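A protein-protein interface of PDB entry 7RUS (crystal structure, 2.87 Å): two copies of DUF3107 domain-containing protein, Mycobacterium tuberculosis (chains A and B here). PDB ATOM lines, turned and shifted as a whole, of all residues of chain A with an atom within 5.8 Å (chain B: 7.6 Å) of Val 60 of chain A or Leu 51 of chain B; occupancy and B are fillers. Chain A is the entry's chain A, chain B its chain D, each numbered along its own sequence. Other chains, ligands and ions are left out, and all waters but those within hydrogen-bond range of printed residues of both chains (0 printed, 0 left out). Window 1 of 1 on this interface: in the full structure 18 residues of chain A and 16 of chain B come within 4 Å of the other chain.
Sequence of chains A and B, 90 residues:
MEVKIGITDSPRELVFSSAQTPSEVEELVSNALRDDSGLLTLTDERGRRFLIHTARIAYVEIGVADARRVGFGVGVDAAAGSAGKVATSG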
ATOM      1  N   VAL A   3       4.862 -24.922 -17.573  1.00  0.00           N
ATOM      2  CA  VAL A   3       5.424 -23.664 -17.941  1.00  0.00           C
ATOM      3  C   VAL A   3       6.112 -23.915 -19.277  1.00  0.00           C
ATOM      4  O   VAL A   3       6.945 -24.820 -19.413  1.00  0.00           O
ATOM      5  CB  VAL A   3       6.390 -23.156 -16.880  1.00  0.00           C
ATOM      6  CG1 VAL A   3       6.896 -21.770 -17.215  1.00  0.00           C
ATOM      7  CG2 VAL A   3       5.693 -23.114 -15.547  1.00  0.00           C
ATOM      8  N   LYS A   4       5.707 -23.132 -20.278  1.00  0.00           N
ATOM      9  CA  LYS A   4       6.368 -23.118 -21.560  1.00  0.00           C
ATOM     10  C   LYS A   4       7.031 -21.765 -21.738  1.00  0.00           C
ATOM     11  O   LYS A   4       6.398 -20.749 -21.509  1.00  0.00           O
ATOM     12  CB  LYS A   4       5.354 -23.359 -22.663  1.00  0.00           C
ATOM     13  CG  LYS A   4       4.737 -24.738 -22.589  1.00  0.00           C
ATOM     14  CD  LYS A   4       4.022 -25.129 -23.840  1.00  0.00           C
ATOM     15  CE  LYS A   4       3.285 -26.427 -23.591  1.00  0.00           C
ATOM     16  NZ  LYS A   4       2.238 -26.576 -24.642  1.00  0.00           N
ATOM     17  N   ILE A   5       8.307 -21.764 -22.123  1.00  0.00           N
ATOM     18  CA  ILE A   5       9.044 -20.544 -22.380  1.00  0.00           C
ATOM     19  C   ILE A   5       9.600 -20.606 -23.785  1.00  0.00           C
ATOM     20  O   ILE A   5      10.363 -21.505 -24.125  1.00  0.00           O
ATOM     21  CB  ILE A   5      10.205 -20.367 -21.395  1.00  0.00           C
ATOM     22  CG1 ILE A   5       9.666 -20.339 -19.966  1.00  0.00           C
ATOM     23  CG2 ILE A   5      10.938 -19.070 -21.696  1.00  0.00           C
ATOM     24  CD1 ILE A   5      10.604 -20.818 -18.926  1.00  0.00           C
ATOM     25  N   GLY A   6       9.165 -19.659 -24.614  1.00  0.00           N
ATOM     26  CA  GLY A   6       9.671 -19.491 -25.943  1.00  0.00           C
ATOM     27  C   GLY A   6      10.876 -18.591 -25.935  1.00  0.00           C
ATOM     28  O   GLY A   6      10.892 -17.564 -25.292  1.00  0.00           O
ATOM     29  N   VAL A  25       5.317 -17.893 -10.234  1.00  0.00           N
ATOM     30  CA  VAL A  25       6.019 -17.911 -11.504  1.00  0.00           C
ATOM     31  C   VAL A  25       5.802 -16.612 -12.271  1.00  0.00           C
ATOM     32  O   VAL A  25       6.756 -16.056 -12.822  1.00  0.00           O
ATOM     33  CB  VAL A  25       5.624 -19.108 -12.373  1.00  0.00           C
ATOM     34  CG1 VAL A  25       6.332 -19.030 -13.727  1.00  0.00           C
ATOM     35  CG2 VAL A  25       5.970 -20.399 -11.649  1.00  0.00           C
ATOM     36  N   GLU A  26       4.560 -16.123 -12.291  1.00  0.00           N
ATOM     37  CA  GLU A  26       4.243 -14.849 -12.930  1.00  0.00           C
ATOM     38  C   GLU A  26       5.040 -13.691 -12.344  1.00  0.00           C
ATOM     39  O   GLU A  26       5.557 -12.890 -13.051  1.00  0.00           O
ATOM     40  CB  GLU A  26       2.751 -14.550 -12.855  1.00  0.00           C
ATOM     41  CG  GLU A  26       2.366 -13.219 -13.454  1.00  0.00           C
ATOM     42  CD  GLU A  26       0.847 -13.048 -13.571  1.00  0.00           C
ATOM     43  OE1 GLU A  26       0.049 -13.817 -13.012  1.00  0.00           O
ATOM     44  OE2 GLU A  26       0.405 -12.101 -14.223  1.00  0.00           O
ATOM     45  N   VAL A  29       8.770 -14.013 -13.515  1.00  0.00           N
ATOM     46  CA  VAL A  29       8.874 -13.654 -14.919  1.00  0.00           C
ATOM     47  C   VAL A  29       8.648 -12.159 -15.161  1.00  0.00           C
ATOM     48  O   VAL A  29       9.432 -11.495 -15.866  1.00  0.00           O
ATOM     49  CB  VAL A  29       7.889 -14.455 -15.758  1.00  0.00           C
ATOM     50  CG1 VAL A  29       7.877 -13.970 -17.180  1.00  0.00           C
ATOM     51  CG2 VAL A  29       8.270 -15.936 -15.736  1.00  0.00           C
ATOM     52  N   SER A  30       7.575 -11.629 -14.581  1.00  0.00           N
ATOM     53  CA  SER A  30       7.193 -10.222 -14.732  1.00  0.00           C
ATOM     54  C   SER A  30       8.292  -9.341 -14.273  1.00  0.00           C
ATOM     55  O   SER A  30       8.622  -8.408 -14.968  1.00  0.00           O
ATOM     56  CB  SER A  30       5.955  -9.857 -13.924  1.00  0.00           C
ATOM     57  OG  SER A  30       4.913 -10.738 -14.258  1.00  0.00           O
ATOM     58  N   LEU A  33      11.208  -9.411 -16.875  1.00  0.00           N
ATOM     59  CA  LEU A  33      10.859  -8.633 -18.058  1.00  0.00           C
ATOM     60  C   LEU A  33      10.769  -7.111 -17.799  1.00  0.00           C
ATOM     61  O   LEU A  33      11.407  -6.337 -18.475  1.00  0.00           O
ATOM     62  CB  LEU A  33       9.558  -9.176 -18.666  1.00  0.00           C
ATOM     63  CG  LEU A  33       9.730 -10.583 -19.282  1.00  0.00           C
ATOM     64  CD1 LEU A  33       8.371 -11.151 -19.680  1.00  0.00           C
ATOM     65  CD2 LEU A  33      10.660 -10.542 -20.490  1.00  0.00           C
ATOM     66  N   LEU A  40      16.816 -14.819 -15.624  1.00  0.00           N
ATOM     67  CA  LEU A  40      15.608 -15.321 -14.989  1.00  0.00           C
ATOM     68  C   LEU A  40      15.884 -16.770 -14.545  1.00  0.00           C
ATOM     69  O   LEU A  40      16.410 -17.576 -15.313  1.00  0.00           O
ATOM     70  CB  LEU A  40      14.437 -15.274 -15.960  1.00  0.00           C
ATOM     71  CG  LEU A  40      13.216 -16.148 -15.650  1.00  0.00           C
ATOM     72  CD1 LEU A  40      12.508 -15.621 -14.397  1.00  0.00           C
ATOM     73  CD2 LEU A  40      12.279 -16.192 -16.851  1.00  0.00           C
ATOM     74  N   LEU A  42      14.197 -20.251 -12.944  1.00  0.00           N
ATOM     75  CA  LEU A  42      13.056 -21.080 -12.596  1.00  0.00           C
ATOM     76  C   LEU A  42      13.500 -22.518 -12.250  1.00  0.00           C
ATOM     77  O   LEU A  42      14.393 -23.072 -12.875  1.00  0.00           O
ATOM     78  CB  LEU A  42      12.049 -21.056 -13.736  1.00  0.00           C
ATOM     79  CG  LEU A  42      11.388 -19.691 -13.925  1.00  0.00           C
ATOM     80  CD1 LEU A  42      10.597 -19.609 -15.226  1.00  0.00           C
ATOM     81  CD2 LEU A  42      10.490 -19.319 -12.746  1.00  0.00           C
ATOM     82  N   ILE A  57      13.882 -13.925 -24.090  1.00  0.00           N
ATOM     83  CA  ILE A  57      12.533 -14.468 -23.918  1.00  0.00           C
ATOM     84  C   ILE A  57      11.556 -13.866 -24.931  1.00  0.00           C
ATOM     85  O   ILE A  57      11.442 -12.632 -25.053  1.00  0.00           O
ATOM     86  CB  ILE A  57      12.007 -14.221 -22.494  1.00  0.00           C
ATOM     87  CG1 ILE A  57      12.841 -14.986 -21.481  1.00  0.00           C
ATOM     88  CG2 ILE A  57      10.574 -14.667 -22.373  1.00  0.00           C
ATOM     89  CD1 ILE A  57      12.606 -14.560 -20.066  1.00  0.00           C
ATOM     90  N   ALA A  58      10.856 -14.742 -25.663  1.00  0.00           N
ATOM     91  CA  ALA A  58       9.728 -14.363 -26.522  1.00  0.00           C
ATOM     92  C   ALA A  58       8.462 -14.288 -25.676  1.00  0.00           C
ATOM     93  O   ALA A  58       7.809 -13.246 -25.609  1.00  0.00           O
ATOM     94  CB  ALA A  58       9.538 -15.350 -27.659  1.00  0.00           C
ATOM     95  N   TYR A  59       8.133 -15.383 -24.984  1.00  0.00           N
ATOM     96  CA  TYR A  59       6.929 -15.460 -24.123  1.00  0.00           C
ATOM     97  C   TYR A  59       7.120 -16.521 -23.043  1.00  0.00           C
ATOM     98  O   TYR A  59       7.950 -17.401 -23.223  1.00  0.00           O
ATOM     99  CB  TYR A  59       5.686 -15.837 -24.932  1.00  0.00           C
ATOM    100  CG  TYR A  59       5.836 -17.138 -25.678  1.00  0.00           C
ATOM    101  CD1 TYR A  59       5.546 -18.366 -25.097  1.00  0.00           C
ATOM    102  CD2 TYR A  59       6.329 -17.134 -26.965  1.00  0.00           C
ATOM    103  CE1 TYR A  59       5.767 -19.551 -25.777  1.00  0.00           C
ATOM    104  CE2 TYR A  59       6.472 -18.309 -27.693  1.00  0.00           C
ATOM    105  CZ  TYR A  59       6.213 -19.517 -27.083  1.00  0.00           C
ATOM    106  OH  TYR A  59       6.387 -20.683 -27.758  1.00  0.00           O
ATOM    107  N   VAL A  60       6.302 -16.443 -21.996  1.00  0.00           N
ATOM    108  CA  VAL A  60       6.022 -17.538 -21.094  1.00  0.00           C
ATOM    109  C   VAL A  60       4.519 -17.812 -21.051  1.00  0.00           C
ATOM    110  O   VAL A  60       3.731 -16.925 -20.843  1.00  0.00           O
ATOM    111  CB  VAL A  60       6.500 -17.196 -19.668  1.00  0.00           C
ATOM    112  CG1 VAL A  60       6.374 -18.411 -18.762  1.00  0.00           C
ATOM    113  CG2 VAL A  60       7.921 -16.637 -19.711  1.00  0.00           C
ATOM    114  N   GLU A  61       4.140 -19.065 -21.279  1.00  0.00           N
ATOM    115  CA  GLU A  61       2.807 -19.581 -21.001  1.00  0.00           C
ATOM    116  C   GLU A  61       2.873 -20.317 -19.654  1.00  0.00           C
ATOM    117  O   GLU A  61       3.659 -21.234 -19.473  1.00  0.00           O
ATOM    118  CB  GLU A  61       2.348 -20.513 -22.117  1.00  0.00           C
ATOM    119  CG  GLU A  61       1.210 -21.474 -21.765  1.00  0.00           C
ATOM    120  CD  GLU A  61       0.797 -22.395 -22.942  1.00  0.00           C
ATOM    121  OE1 GLU A  61       1.485 -22.438 -23.995  1.00  0.00           O
ATOM    122  OE2 GLU A  61      -0.242 -23.090 -22.817  1.00  0.00           O
ATOM    123  N   ILE A  62       2.057 -19.853 -18.703  1.00  0.00           N
ATOM    124  CA  ILE A  62       1.831 -20.487 -17.430  1.00  0.00           C
ATOM    125  C   ILE A  62       0.500 -21.207 -17.512  1.00  0.00           C
ATOM    126  O   ILE A  62      -0.520 -20.623 -17.826  1.00  0.00           O
ATOM    127  CB  ILE A  62       1.756 -19.466 -16.298  1.00  0.00           C
ATOM    128  CG1 ILE A  62       3.080 -18.695 -16.196  1.00  0.00           C
ATOM    129  CG2 ILE A  62       1.508 -20.156 -14.964  1.00  0.00           C
ATOM    130  CD1 ILE A  62       2.993 -17.410 -15.389  1.00  0.00           C
ATOM    131  N   ARG B  12       6.395 -20.826 -33.232  1.00  0.00           N
ATOM    132  CA  ARG B  12       5.005 -20.950 -32.699  1.00  0.00           C
ATOM    133  C   ARG B  12       4.245 -19.625 -32.814  1.00  0.00           C
ATOM    134  O   ARG B  12       4.845 -18.564 -32.579  1.00  0.00           O
ATOM    135  CB  ARG B  12       5.031 -21.376 -31.226  1.00  0.00           C
ATOM    136  CG  ARG B  12       3.661 -21.663 -30.637  1.00  0.00           C
ATOM    137  CD  ARG B  12       3.738 -22.188 -29.225  1.00  0.00           C
ATOM    138  NE  ARG B  12       2.433 -22.109 -28.576  1.00  0.00           N
ATOM    139  CZ  ARG B  12       2.215 -22.187 -27.273  1.00  0.00           C
ATOM    140  NH1 ARG B  12       3.199 -22.361 -26.408  1.00  0.00           N
ATOM    141  NH2 ARG B  12       0.982 -22.076 -26.829  1.00  0.00           N
ATOM    142  N   LEU B  14       1.109 -17.966 -30.971  1.00  0.00           N
ATOM    143  CA  LEU B  14       0.285 -18.196 -29.806  1.00  0.00           C
ATOM    144  C   LEU B  14      -1.169 -18.046 -30.202  1.00  0.00           C
ATOM    145  O   LEU B  14      -1.537 -17.089 -30.862  1.00  0.00           O
ATOM    146  CB  LEU B  14       0.597 -17.174 -28.734  1.00  0.00           C
ATOM    147  CG  LEU B  14       1.998 -17.205 -28.184  1.00  0.00           C
ATOM    148  CD1 LEU B  14       2.132 -16.137 -27.123  1.00  0.00           C
ATOM    149  CD2 LEU B  14       2.283 -18.546 -27.573  1.00  0.00           C
ATOM    150  N   GLY B  38       7.357  -3.663 -22.560  1.00  0.00           N
ATOM    151  CA  GLY B  38       8.320  -4.659 -22.080  1.00  0.00           C
ATOM    152  C   GLY B  38       7.745  -5.906 -21.445  1.00  0.00           C
ATOM    153  O   GLY B  38       8.469  -6.905 -21.448  1.00  0.00           O
ATOM    154  N   LEU B  39       6.441  -5.916 -21.133  1.00  0.00           N
ATOM    155  CA  LEU B  39       5.669  -7.127 -20.807  1.00  0.00           C
ATOM    156  C   LEU B  39       4.183  -6.889 -21.105  1.00  0.00           C
ATOM    157  O   LEU B  39       3.633  -5.897 -20.686  1.00  0.00           O
ATOM    158  CB  LEU B  39       5.834  -7.449 -19.337  1.00  0.00           C
ATOM    159  CG  LEU B  39       4.879  -8.434 -18.632  1.00  0.00           C
ATOM    160  CD1 LEU B  39       5.100  -9.853 -19.105  1.00  0.00           C
ATOM    161  CD2 LEU B  39       5.078  -8.353 -17.122  1.00  0.00           C
ATOM    162  N   LEU B  40       3.567  -7.795 -21.862  1.00  0.00           N
ATOM    163  CA  LEU B  40       2.140  -7.824 -22.108  1.00  0.00           C
ATOM    164  C   LEU B  40       1.591  -9.107 -21.492  1.00  0.00           C
ATOM    165  O   LEU B  40       2.141 -10.204 -21.673  1.00  0.00           O
ATOM    166  CB  LEU B  40       1.862  -7.822 -23.614  1.00  0.00           C
ATOM    167  CG  LEU B  40       0.470  -8.236 -24.082  1.00  0.00           C
ATOM    168  CD1 LEU B  40      -0.596  -7.254 -23.620  1.00  0.00           C
ATOM    169  CD2 LEU B  40       0.428  -8.350 -25.589  1.00  0.00           C
ATOM    170  N   THR B  41       0.487  -8.985 -20.748  1.00  0.00           N
ATOM    171  CA  THR B  41      -0.118 -10.127 -20.078  1.00  0.00           C
ATOM    172  C   THR B  41      -1.537 -10.343 -20.572  1.00  0.00           C
ATOM    173  O   THR B  41      -2.373  -9.459 -20.459  1.00  0.00           O
ATOM    174  CB  THR B  41      -0.075  -9.973 -18.553  1.00  0.00           C
ATOM    175  OG1 THR B  41       1.281  -9.762 -18.164  1.00  0.00           O
ATOM    176  CG2 THR B  41      -0.599 -11.221 -17.848  1.00  0.00           C
ATOM    177  N   LEU B  42      -1.778 -11.549 -21.109  1.00  0.00           N
ATOM    178  CA  LEU B  42      -3.089 -11.985 -21.506  1.00  0.00           C
ATOM    179  C   LEU B  42      -3.478 -13.321 -20.825  1.00  0.00           C
ATOM    180  O   LEU B  42      -2.658 -14.189 -20.632  1.00  0.00           O
ATOM    181  CB  LEU B  42      -3.122 -12.088 -23.025  1.00  0.00           C
ATOM    182  CG  LEU B  42      -3.077 -10.722 -23.716  1.00  0.00           C
ATOM    183  CD1 LEU B  42      -2.875 -10.845 -25.224  1.00  0.00           C
ATOM    184  CD2 LEU B  42      -4.336  -9.905 -23.417  1.00  0.00           C
ATOM    185  N   THR B  43      -4.755 -13.464 -20.480  1.00  0.00           N
ATOM    186  CA  THR B  43      -5.273 -14.671 -19.901  1.00  0.00           C
ATOM    187  C   THR B  43      -6.347 -15.253 -20.789  1.00  0.00           C
ATOM    188  O   THR B  43      -7.068 -14.531 -21.435  1.00  0.00           O
ATOM    189  CB  THR B  43      -5.856 -14.410 -18.504  1.00  0.00           C
ATOM    190  OG1 THR B  43      -6.812 -13.359 -18.569  1.00  0.00           O
ATOM    191  CG2 THR B  43      -4.755 -14.028 -17.587  1.00  0.00           C
ATOM    192  N   ARG B  48      -5.133 -19.925 -18.306  1.00  0.00           N
ATOM    193  CA  ARG B  48      -3.722 -19.934 -18.767  1.00  0.00           C
ATOM    194  C   ARG B  48      -3.248 -18.495 -18.921  1.00  0.00           C
ATOM    195  O   ARG B  48      -4.027 -17.670 -19.443  1.00  0.00           O
ATOM    196  CB  ARG B  48      -3.566 -20.622 -20.119  1.00  0.00           C
ATOM    197  CG  ARG B  48      -3.639 -22.139 -20.074  1.00  0.00           C
ATOM    198  CD  ARG B  48      -3.136 -22.675 -21.400  1.00  0.00           C
ATOM    199  NE  ARG B  48      -4.001 -22.178 -22.450  1.00  0.00           N
ATOM    200  CZ  ARG B  48      -3.756 -22.225 -23.747  1.00  0.00           C
ATOM    201  NH1 ARG B  48      -2.617 -22.719 -24.192  1.00  0.00           N
ATOM    202  NH2 ARG B  48      -4.642 -21.738 -24.601  1.00  0.00           N
ATOM    203  N   ARG B  49      -2.011 -18.226 -18.516  1.00  0.00           N
ATOM    204  CA  ARG B  49      -1.390 -16.879 -18.555  1.00  0.00           C
ATOM    205  C   ARG B  49      -0.316 -16.832 -19.639  1.00  0.00           C
ATOM    206  O   ARG B  49       0.563 -17.675 -19.623  1.00  0.00           O
ATOM    207  CB  ARG B  49      -0.764 -16.551 -17.197  1.00  0.00           C
ATOM    208  CG  ARG B  49      -1.778 -16.181 -16.130  1.00  0.00           C
ATOM    209  CD  ARG B  49      -1.255 -16.478 -14.732  1.00  0.00           C
ATOM    210  NE  ARG B  49      -2.328 -16.864 -13.835  1.00  0.00           N
ATOM    211  CZ  ARG B  49      -2.383 -16.559 -12.539  1.00  0.00           C
ATOM    212  NH1 ARG B  49      -1.441 -15.831 -11.966  1.00  0.00           N
ATOM    213  NH2 ARG B  49      -3.400 -16.968 -11.813  1.00  0.00           N
ATOM    214  N   PHE B  50      -0.410 -15.865 -20.542  1.00  0.00           N
ATOM    215  CA  PHE B  50       0.621 -15.589 -21.524  1.00  0.00           C
ATOM    216  C   PHE B  50       1.282 -14.282 -21.170  1.00  0.00           C
ATOM    217  O   PHE B  50       0.617 -13.257 -21.125  1.00  0.00           O
ATOM    218  CB  PHE B  50       0.030 -15.514 -22.920  1.00  0.00           C
ATOM    219  CG  PHE B  50      -0.569 -16.791 -23.372  1.00  0.00           C
ATOM    220  CD1 PHE B  50      -1.902 -17.081 -23.128  1.00  0.00           C
ATOM    221  CD2 PHE B  50       0.215 -17.728 -24.023  1.00  0.00           C
ATOM    222  CE1 PHE B  50      -2.438 -18.279 -23.535  1.00  0.00           C
ATOM    223  CE2 PHE B  50      -0.313 -18.931 -24.452  1.00  0.00           C
ATOM    224  CZ  PHE B  50      -1.629 -19.208 -24.201  1.00  0.00           C
ATOM    225  N   LEU B  51       2.579 -14.360 -20.883  1.00  0.00           N
ATOM    226  CA  LEU B  51       3.429 -13.214 -20.610  1.00  0.00           C
ATOM    227  C   LEU B  51       4.317 -13.095 -21.829  1.00  0.00           C
ATOM    228  O   LEU B  51       5.129 -13.948 -22.065  1.00  0.00           O
ATOM    229  CB  LEU B  51       4.261 -13.468 -19.361  1.00  0.00           C
ATOM    230  CG  LEU B  51       3.527 -13.341 -18.027  1.00  0.00           C
ATOM    231  CD1 LEU B  51       2.286 -14.214 -17.982  1.00  0.00           C
ATOM    232  CD2 LEU B  51       4.401 -13.694 -16.833  1.00  0.00           C
ATOM    233  N   ILE B  52       4.122 -12.036 -22.611  1.00  0.00           N
ATOM    234  CA  ILE B  52       4.812 -11.845 -23.869  1.00  0.00           C
ATOM    235  C   ILE B  52       5.696 -10.633 -23.767  1.00  0.00           C
ATOM    236  O   ILE B  52       5.349  -9.657 -23.128  1.00  0.00           O
ATOM    237  CB  ILE B  52       3.804 -11.648 -25.005  1.00  0.00           C
ATOM    238  CG1 ILE B  52       2.893 -12.878 -25.097  1.00  0.00           C
ATOM    239  CG2 ILE B  52       4.528 -11.444 -26.326  1.00  0.00           C
ATOM    240  CD1 ILE B  52       1.428 -12.548 -25.167  1.00  0.00           C
ATOM    241  N   HIS B  53       6.868 -10.726 -24.383  1.00  0.00           N
ATOM    242  CA  HIS B  53       7.855  -9.665 -24.395  1.00  0.00           C
ATOM    243  C   HIS B  53       7.451  -8.702 -25.518  1.00  0.00           C
ATOM    244  O   HIS B  53       7.659  -8.999 -26.688  1.00  0.00           O
ATOM    245  CB  HIS B  53       9.215 -10.309 -24.666  1.00  0.00           C
ATOM    246  CG  HIS B  53      10.378  -9.408 -24.447  1.00  0.00           C
ATOM    247  ND1 HIS B  53      11.677  -9.879 -24.441  1.00  0.00           N
ATOM    248  CD2 HIS B  53      10.440  -8.087 -24.174  1.00  0.00           C
ATOM    249  CE1 HIS B  53      12.501  -8.874 -24.226  1.00  0.00           C
ATOM    250  NE2 HIS B  53      11.776  -7.779 -24.037  1.00  0.00           N
ATOM    251  N   THR B  54       6.849  -7.562 -25.154  1.00  0.00           N
ATOM    252  CA  THR B  54       6.148  -6.682 -26.113  1.00  0.00           C
ATOM    253  C   THR B  54       6.941  -6.445 -27.393  1.00  0.00           C
ATOM    254  O   THR B  54       6.402  -6.482 -28.500  1.00  0.00           O
ATOM    255  CB  THR B  54       5.866  -5.299 -25.504  1.00  0.00           C
ATOM    256  OG1 THR B  54       5.158  -5.445 -24.268  1.00  0.00           O
ATOM    257  CG2 THR B  54       5.026  -4.444 -26.441  1.00  0.00           C
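Among the printed residues, pairs that only touch across the chains: Lys 4 of chain A with Arg 12 of chain B (3.9 Å), Glu 26 of chain A with Thr 41 of chain B (3.9 Å), Glu 26 of chain A with Leu 51 of chain B (3.97 Å), Val 29 of chain A with Leu 51 of chain B (3.5 Å), Ser 30 of chain A with Leu 39 of chain B (3.6 Å), Ser 30 of chain A with Leu 51 of chain B (3.95 Å), Leu 33 of chain A with Gly 38 of chain B (3.8 Å), Leu 33 of chain A with Leu 39 of chain B (3.6 Å), Ala 58 of chain A with Ile 52 of chain B (3.7 Å), Tyr 59 of chain A with Arg 12 of chain B (3.4 Å), Tyr 59 of chain A with Leu 51 of chain B (3.1 Å), Val 60 of chain A with Phe 50 of chain B (3.5 Å), Glu 61 of chain A with Arg 49 of chain B (3.3 Å), Glu 61 of chain A with Phe 50 of chain B (3.9 Å) and Ile 62 of chain A with Arg 48 of chain B (3.4 Å).
2 positions are printed for both chains. Of the 23 pairs that touch across the chains among the printed residues, none has its exchanged pair printed and touching as well.
Of the 15 printed residues of chain B, 10 touch a printed residue of chain A. Printed residues of chain B that touch a printed residue of chain A: Arg 12, Gly 38, Leu 39, Thr 41, Arg 48, Arg 49, Phe 50, Leu 51, Ile 52 and His 53. Hydrophobic or aromatic side chains of chain B within 4 Å of the printed part of chain A: Leu 39, Phe 50, Leu 51, Ile 52 and His 53. Of the 17 printed residues of chain A, 11 touch a printed residue of chain B. Hydrophobic or aromatic side chains of chain A within 4 Å of the printed part of chain B: Val 29, Leu 33, Tyr 59 and Ile 62. Among the printed residues, 23 pairs touch across the chains. Among the printed residues, Asp or Glu carboxylates within 4 Å of a Lys or Arg side-chain nitrogen of the other chain: Glu 26 of chain A with Arg 49 of chain B (2.7 Å), Glu 61 of chain A with Arg 12 of chain B (2.9 Å) and Glu 61 of chain A with Arg 48 of chain B (2.8 Å).
The backbone NH of Glu 61 of chain A is in hydrogen-bond range of the backbone carbonyl oxygen of Lys 4 of chain A (2.8 Å). The backbone NH (N) of Ala 58 of chain A lies within hydrogen-bond range of the backbone carbonyl oxygen (O) of Gly 6 of chain A (2.8 Å). The backbone NH of Gly 6 of chain A lies within hydrogen-bond range of the backbone carbonyl oxygen of Tyr 59 of chain A (2.9 Å). N of Gly 38 of chain B sits at hydrogen-bond distance from OG1 of Thr 54 of chain B (3.3 Å). The backbone NH (N) of Leu 39 of chain B is in hydrogen-bond range of the side-chain hydroxyl (OG1) of Thr 54 of chain B (3.4 Å). The backbone carbonyl oxygen of Leu 40 of chain B sits at hydrogen-bond distance from the backbone NH of Ile 52 of chain B, 2.9 Å away.
Val 3 of chain A touches none of the printed residues of chain B. Of the printed residues of chain B, Glu 26 of chain A touches Thr 41, Arg 49 and Leu 51. Of the printed residues of chain B, Tyr 59 of chain A touches Arg 12 (3.4 Å) and Leu 51 (3.1 Å). Val 60 of chain A touches three residues of chain B. Of the printed residues of chain A, Gly 38 of chain B touches Leu 33. Of the printed residues of chain A, Leu 39 of chain B touches Ser 30 and Leu 33. Leu 42 of chain B touches none of the printed residues of chain A. Of the printed residues of chain A, Arg 48 of chain B touches Glu 61 and Ile 62. Leu 51 of chain B touches just these residues of chain A: Glu 26 (3.97 Å), Val 29 (3.5 Å), Ser 30 (3.95 Å), Tyr 59 (3.1 Å) and Val 60 (2.8 Å).
The side-chain carboxylate of Glu 26 of chain A is in salt-bridge range of the guanidinium group of Arg 49 of chain B, 2.7 Å away. The backbone carbonyl oxygen (O) of Ile 57 of chain A is in hydrogen-bond range of a ring nitrogen (ND1) of His 53 of chain B. N of His 53 of chain B lies within hydrogen-bond range of O of Ala 58 of chain A (3.0 Å). O of Leu 51 of chain B lies within hydrogen-bond range of N of Val 60 of chain A (2.8 Å). OE1 of Glu 61 of chain A lies within salt-bridge range of NH2 of Arg 12 of chain B, 2.9 Å away. The guanidinium group (NH1) of Arg 48 of chain B lies within salt-bridge range of the side-chain carboxylate (OE2) of Glu 61 of chain A, at 2.8 Å. The backbone NH (N) of Ile 62 of chain A is in hydrogen-bond range of the backbone carbonyl oxygen (O) of Arg 49 of chain B (2.8 Å). The backbone carbonyl oxygen of Arg 49 of chain B lies close to the backbone carbonyl oxygen of Val 60 of chain A (3.5 Å).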
